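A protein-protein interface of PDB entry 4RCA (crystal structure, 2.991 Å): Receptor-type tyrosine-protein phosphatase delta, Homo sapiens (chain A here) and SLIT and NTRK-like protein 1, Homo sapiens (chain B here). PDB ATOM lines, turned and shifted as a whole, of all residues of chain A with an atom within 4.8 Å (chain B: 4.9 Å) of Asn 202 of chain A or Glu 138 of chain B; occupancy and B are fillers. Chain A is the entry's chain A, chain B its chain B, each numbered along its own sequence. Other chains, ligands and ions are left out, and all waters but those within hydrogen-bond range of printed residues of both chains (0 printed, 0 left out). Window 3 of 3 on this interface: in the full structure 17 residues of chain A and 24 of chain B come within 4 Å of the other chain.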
ATOM      1  N   GLN A 113       6.033   7.375  -1.027  1.00  0.00           N
ATOM      2  CA  GLN A 113       5.646   6.541   0.104  1.00  0.00           C
ATOM      3  C   GLN A 113       4.399   7.079   0.794  1.00  0.00           C
ATOM      4  O   GLN A 113       3.942   8.182   0.493  1.00  0.00           O
ATOM      5  CB  GLN A 113       6.796   6.446   1.109  1.00  0.00           C
ATOM      6  CG  GLN A 113       8.032   5.746   0.575  1.00  0.00           C
ATOM      7  CD  GLN A 113       7.868   4.242   0.516  1.00  0.00           C
ATOM      8  OE1 GLN A 113       7.766   3.576   1.547  1.00  0.00           O
ATOM      9  NE2 GLN A 113       7.839   3.696  -0.694  1.00  0.00           N
ATOM     10  N   LEU A 114       3.850   6.293   1.715  1.00  0.00           N
ATOM     11  CA  LEU A 114       2.746   6.757   2.545  1.00  0.00           C
ATOM     12  C   LEU A 114       3.233   7.913   3.405  1.00  0.00           C
ATOM     13  O   LEU A 114       4.356   7.887   3.912  1.00  0.00           O
ATOM     14  CB  LEU A 114       2.193   5.628   3.419  1.00  0.00           C
ATOM     15  CG  LEU A 114       1.002   5.975   4.318  1.00  0.00           C
ATOM     16  CD1 LEU A 114      -0.016   4.851   4.309  1.00  0.00           C
ATOM     17  CD2 LEU A 114       1.451   6.270   5.745  1.00  0.00           C
ATOM     18  N   LYS A 115       2.393   8.927   3.568  1.00  0.00           N
ATOM     19  CA  LYS A 115       2.808  10.126   4.278  1.00  0.00           C
ATOM     20  C   LYS A 115       1.672  10.732   5.090  1.00  0.00           C
ATOM     21  O   LYS A 115       0.625  11.086   4.548  1.00  0.00           O
ATOM     22  CB  LYS A 115       3.353  11.156   3.287  1.00  0.00           C
ATOM     23  CG  LYS A 115       4.497  11.996   3.825  1.00  0.00           C
ATOM     24  CD  LYS A 115       5.147  12.807   2.717  1.00  0.00           C
ATOM     25  CE  LYS A 115       6.525  13.293   3.132  1.00  0.00           C
ATOM     26  NZ  LYS A 115       7.423  12.154   3.474  1.00  0.00           N
ATOM     27  N   GLY A 183      -4.820  12.361  -0.253  1.00  0.00           N
ATOM     28  CA  GLY A 183      -5.378  11.515  -1.296  1.00  0.00           C
ATOM     29  C   GLY A 183      -4.319  10.641  -1.947  1.00  0.00           C
ATOM     30  O   GLY A 183      -3.167  10.638  -1.518  1.00  0.00           O
ATOM     31  N   LYS A 184      -4.705   9.910  -2.989  1.00  0.00           N
ATOM     32  CA  LYS A 184      -3.813   8.930  -3.604  1.00  0.00           C
ATOM     33  C   LYS A 184      -2.966   9.533  -4.725  1.00  0.00           C
ATOM     34  O   LYS A 184      -3.484   9.911  -5.775  1.00  0.00           O
ATOM     35  CB  LYS A 184      -4.625   7.749  -4.141  1.00  0.00           C
ATOM     36  CG  LYS A 184      -3.798   6.508  -4.416  1.00  0.00           C
ATOM     37  CD  LYS A 184      -4.673   5.334  -4.837  1.00  0.00           C
ATOM     38  CE  LYS A 184      -5.633   4.911  -3.731  1.00  0.00           C
ATOM     39  NZ  LYS A 184      -6.381   3.668  -4.086  1.00  0.00           N
ATOM     40  N   PRO A 200       0.890   3.523  -6.105  1.00  0.00           N
ATOM     41  CA  PRO A 200       0.159   4.629  -5.480  1.00  0.00           C
ATOM     42  C   PRO A 200       0.603   4.877  -4.042  1.00  0.00           C
ATOM     43  O   PRO A 200       0.929   3.936  -3.318  1.00  0.00           O
ATOM     44  CB  PRO A 200      -1.297   4.160  -5.532  1.00  0.00           C
ATOM     45  CG  PRO A 200      -1.209   2.677  -5.553  1.00  0.00           C
ATOM     46  CD  PRO A 200       0.022   2.360  -6.354  1.00  0.00           C
ATOM     47  N   ALA A 201       0.618   6.146  -3.650  1.00  0.00           N
ATOM     48  CA  ALA A 201       1.025   6.539  -2.309  1.00  0.00           C
ATOM     49  C   ALA A 201      -0.037   7.419  -1.667  1.00  0.00           C
ATOM     50  O   ALA A 201      -0.333   8.510  -2.158  1.00  0.00           O
ATOM     51  CB  ALA A 201       2.357   7.263  -2.347  1.00  0.00           C
ATOM     52  N   ASN A 202      -0.610   6.936  -0.569  1.00  0.00           N
ATOM     53  CA  ASN A 202      -1.591   7.709   0.177  1.00  0.00           C
ATOM     54  C   ASN A 202      -0.944   8.865   0.926  1.00  0.00           C
ATOM     55  O   ASN A 202       0.087   8.701   1.578  1.00  0.00           O
ATOM     56  CB  ASN A 202      -2.348   6.818   1.167  1.00  0.00           C
ATOM     57  CG  ASN A 202      -3.344   5.899   0.488  1.00  0.00           C
ATOM     58  OD1 ASN A 202      -3.656   6.060  -0.691  1.00  0.00           O
ATOM     59  ND2 ASN A 202      -3.861   4.933   1.239  1.00  0.00           N
ATOM     60  N   LEU A 203      -1.554  10.038   0.811  1.00  0.00           N
ATOM     61  CA  LEU A 203      -1.186  11.180   1.630  1.00  0.00           C
ATOM     62  C   LEU A 203      -2.302  11.423   2.631  1.00  0.00           C
ATOM     63  O   LEU A 203      -3.468  11.544   2.247  1.00  0.00           O
ATOM     64  CB  LEU A 203      -0.950  12.426   0.774  1.00  0.00           C
ATOM     65  CG  LEU A 203      -0.605  13.697   1.555  1.00  0.00           C
ATOM     66  CD1 LEU A 203       0.709  13.528   2.303  1.00  0.00           C
ATOM     67  CD2 LEU A 203      -0.553  14.913   0.642  1.00  0.00           C
ATOM     68  N   TYR A 204      -1.948  11.465   3.912  1.00  0.00           N
ATOM     69  CA  TYR A 204      -2.909  11.778   4.965  1.00  0.00           C
ATOM     70  C   TYR A 204      -2.562  13.119   5.603  1.00  0.00           C
ATOM     71  O   TYR A 204      -1.395  13.504   5.658  1.00  0.00           O
ATOM     72  CB  TYR A 204      -2.942  10.676   6.029  1.00  0.00           C
ATOM     73  CG  TYR A 204      -3.522   9.354   5.563  1.00  0.00           C
ATOM     74  CD1 TYR A 204      -4.896   9.148   5.528  1.00  0.00           C
ATOM     75  CD2 TYR A 204      -2.695   8.305   5.179  1.00  0.00           C
ATOM     76  CE1 TYR A 204      -5.431   7.939   5.110  1.00  0.00           C
ATOM     77  CE2 TYR A 204      -3.221   7.092   4.763  1.00  0.00           C
ATOM     78  CZ  TYR A 204      -4.587   6.915   4.729  1.00  0.00           C
ATOM     79  OH  TYR A 204      -5.108   5.710   4.313  1.00  0.00           O
ATOM     80  N   GLU B 114      -8.250   1.641   8.119  1.00  0.00           N
ATOM     81  CA  GLU B 114      -6.878   1.840   7.661  1.00  0.00           C
ATOM     82  C   GLU B 114      -6.146   2.871   8.511  1.00  0.00           C
ATOM     83  O   GLU B 114      -4.918   2.860   8.607  1.00  0.00           O
ATOM     84  CB  GLU B 114      -6.858   2.285   6.196  1.00  0.00           C
ATOM     85  CG  GLU B 114      -7.355   1.248   5.209  1.00  0.00           C
ATOM     86  CD  GLU B 114      -7.057   1.632   3.772  1.00  0.00           C
ATOM     87  OE1 GLU B 114      -6.682   2.800   3.534  1.00  0.00           O
ATOM     88  OE2 GLU B 114      -7.189   0.767   2.882  1.00  0.00           O
ATOM     89  N   LYS B 136      -6.044  -3.869   7.643  1.00  0.00           N
ATOM     90  CA  LYS B 136      -5.853  -2.829   6.640  1.00  0.00           C
ATOM     91  C   LYS B 136      -5.279  -1.575   7.289  1.00  0.00           C
ATOM     92  O   LYS B 136      -5.062  -0.562   6.627  1.00  0.00           O
ATOM     93  CB  LYS B 136      -7.167  -2.511   5.927  1.00  0.00           C
ATOM     94  CG  LYS B 136      -7.741  -3.684   5.149  1.00  0.00           C
ATOM     95  CD  LYS B 136      -8.661  -3.212   4.038  1.00  0.00           C
ATOM     96  CE  LYS B 136      -9.031  -4.359   3.112  1.00  0.00           C
ATOM     97  NZ  LYS B 136      -9.418  -3.874   1.757  1.00  0.00           N
ATOM     98  N   LEU B 137      -5.029  -1.668   8.591  1.00  0.00           N
ATOM     99  CA  LEU B 137      -4.517  -0.549   9.372  1.00  0.00           C
ATOM    100  C   LEU B 137      -3.122  -0.134   8.913  1.00  0.00           C
ATOM    101  O   LEU B 137      -2.121  -0.714   9.335  1.00  0.00           O
ATOM    102  CB  LEU B 137      -4.497  -0.916  10.857  1.00  0.00           C
ATOM    103  CG  LEU B 137      -4.483   0.235  11.861  1.00  0.00           C
ATOM    104  CD1 LEU B 137      -5.790   1.009  11.795  1.00  0.00           C
ATOM    105  CD2 LEU B 137      -4.234  -0.287  13.266  1.00  0.00           C
ATOM    106  N   GLU B 138      -3.063   0.871   8.045  1.00  0.00           N
ATOM    107  CA  GLU B 138      -1.792   1.363   7.522  1.00  0.00           C
ATOM    108  C   GLU B 138      -1.140   2.361   8.469  1.00  0.00           C
ATOM    109  O   GLU B 138       0.083   2.388   8.613  1.00  0.00           O
ATOM    110  CB  GLU B 138      -1.989   2.014   6.151  1.00  0.00           C
ATOM    111  CG  GLU B 138      -2.381   1.051   5.044  1.00  0.00           C
ATOM    112  CD  GLU B 138      -2.566   1.748   3.711  1.00  0.00           C
ATOM    113  OE1 GLU B 138      -2.680   1.051   2.682  1.00  0.00           O
ATOM    114  OE2 GLU B 138      -2.599   2.997   3.692  1.00  0.00           O
ATOM    115  N   VAL B 139      -1.963   3.183   9.111  1.00  0.00           N
ATOM    116  CA  VAL B 139      -1.452   4.274   9.931  1.00  0.00           C
ATOM    117  C   VAL B 139      -2.073   4.281  11.329  1.00  0.00           C
ATOM    118  O   VAL B 139      -3.280   4.460  11.501  1.00  0.00           O
ATOM    119  CB  VAL B 139      -1.683   5.633   9.233  1.00  0.00           C
ATOM    120  CG1 VAL B 139      -2.980   5.610   8.445  1.00  0.00           C
ATOM    121  CG2 VAL B 139      -1.646   6.785  10.233  1.00  0.00           C
ATOM    122  N   LEU B 140      -1.212   4.063  12.317  1.00  0.00           N
ATOM    123  CA  LEU B 140      -1.570   4.035  13.727  1.00  0.00           C
ATOM    124  C   LEU B 140      -0.875   5.177  14.467  1.00  0.00           C
ATOM    125  O   LEU B 140       0.359   5.231  14.547  1.00  0.00           O
ATOM    126  CB  LEU B 140      -1.186   2.688  14.343  1.00  0.00           C
ATOM    127  CG  LEU B 140      -1.471   2.475  15.829  1.00  0.00           C
ATOM    128  CD1 LEU B 140      -2.958   2.589  16.101  1.00  0.00           C
ATOM    129  CD2 LEU B 140      -0.940   1.121  16.278  1.00  0.00           C
ATOM    130  N   PRO B 159      -0.774  -4.283   8.723  1.00  0.00           N
ATOM    131  CA  PRO B 159       0.082  -3.602   7.747  1.00  0.00           C
ATOM    132  C   PRO B 159       0.446  -2.180   8.165  1.00  0.00           C
ATOM    133  O   PRO B 159       0.151  -1.232   7.438  1.00  0.00           O
ATOM    134  CB  PRO B 159      -0.779  -3.590   6.484  1.00  0.00           C
ATOM    135  CG  PRO B 159      -2.173  -3.541   7.003  1.00  0.00           C
ATOM    136  CD  PRO B 159      -2.172  -4.367   8.265  1.00  0.00           C
ATOM    137  N   ILE B 160       1.082  -2.043   9.324  1.00  0.00           N
ATOM    138  CA  ILE B 160       1.490  -0.739   9.832  1.00  0.00           C
ATOM    139  C   ILE B 160       2.547  -0.108   8.931  1.00  0.00           C
ATOM    140  O   ILE B 160       3.527  -0.754   8.561  1.00  0.00           O
ATOM    141  CB  ILE B 160       2.044  -0.841  11.268  1.00  0.00           C
ATOM    142  CG1 ILE B 160       1.006  -1.469  12.200  1.00  0.00           C
ATOM    143  CG2 ILE B 160       2.459   0.530  11.782  1.00  0.00           C
ATOM    144  CD1 ILE B 160      -0.210  -0.599  12.437  1.00  0.00           C
ATOM    145  N   THR B 161       2.334   1.156   8.579  1.00  0.00           N
ATOM    146  CA  THR B 161       3.275   1.894   7.748  1.00  0.00           C
ATOM    147  C   THR B 161       3.660   3.197   8.440  1.00  0.00           C
ATOM    148  O   THR B 161       4.783   3.682   8.304  1.00  0.00           O
ATOM    149  CB  THR B 161       2.685   2.195   6.360  1.00  0.00           C
ATOM    150  OG1 THR B 161       1.944   1.059   5.898  1.00  0.00           O
ATOM    151  CG2 THR B 161       3.790   2.518   5.366  1.00  0.00           C
ATOM    152  N   HIS B 162       2.713   3.758   9.184  1.00  0.00           N
ATOM    153  CA  HIS B 162       2.961   4.946   9.989  1.00  0.00           C
ATOM    154  C   HIS B 162       2.697   4.626  11.455  1.00  0.00           C
ATOM    155  O   HIS B 162       1.567   4.374  11.837  1.00  0.00           O
ATOM    156  CB  HIS B 162       2.081   6.109   9.528  1.00  0.00           C
ATOM    157  CG  HIS B 162       2.276   7.369  10.315  1.00  0.00           C
ATOM    158  ND1 HIS B 162       3.107   8.387   9.899  1.00  0.00           N
ATOM    159  CD2 HIS B 162       1.742   7.778  11.491  1.00  0.00           C
ATOM    160  CE1 HIS B 162       3.079   9.366  10.784  1.00  0.00           C
ATOM    161  NE2 HIS B 162       2.258   9.021  11.761  1.00  0.00           N
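The backbone NH (N) of Leu 140 of chain B sits at hydrogen-bond distance from the backbone carbonyl oxygen (O) of His 162 of chain B (2.8 Å). ND2 of Asn 202 of chain A sits at hydrogen-bond distance from OH of Tyr 204 of chain A, at 3.4 Å. The backbone NH (N) of Tyr 204 of chain A is in hydrogen-bond range of the backbone carbonyl oxygen (O) of Lys 115 of chain A, at 2.7 Å. N of Lys 115 of chain A is in hydrogen-bond range of O of Asn 202 of chain A, at 3.1 Å. O of Glu 138 of chain B sits at hydrogen-bond distance from N of Thr 161 of chain B. The backbone carbonyl oxygen (O) of Glu 114 of chain B lies within hydrogen-bond range of the backbone NH (N) of Glu 138 of chain B (2.8 Å).
Asn 202 of chain A touches one residue of chain B. Of the printed residues of chain B, Tyr 204 of chain A touches Glu 114, Glu 138 and Val 139. Of chain A, only Leu 114, Asn 202 and Tyr 204 come within 4 Å of Glu 138 of chain B. Of the printed residues of chain A, Val 139 of chain B touches Tyr 204. Leu 140 of chain B touches none of the printed residues of chain A. Printed residues of chain A within 4 Å of His 162 of chain B: Leu 114.
OE2 of Glu 138 of chain B sits at hydrogen-bond distance from ND2 of Asn 202 of chain A. The side-chain carboxylate of Glu 114 of chain B is in hydrogen-bond range of the side-chain hydroxyl of Tyr 204 of chain A, at 3.4 Å.
Of the 10 printed residues of chain B, 4 touch a printed residue of chain A. Printed residues of chain B that touch a printed residue of chain A: Glu 114, Glu 138, Val 139 and His 162. Along chain B the printed residues that touch a printed residue of chain A span positions 114 to 162. Of the 10 printed residues of chain A, 3 touch a printed residue of chain B. Among the printed residues, 6 pairs touch across the chains. Among the printed residues, no Asp or Glu carboxylate lies within 4 Å of a Lys or Arg side-chain nitrogen of the other chain.
OE2 of Glu 138 of chain B touches CD1 of Leu 114 of chain A, at 3.2 Å. Leu 114 of chain A touches His 162 of chain B. OH of Tyr 204 of chain A touches OE2 of Glu 138 of chain B (3.7 Å). Val 139 of chain B touches Tyr 204 of chain A.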
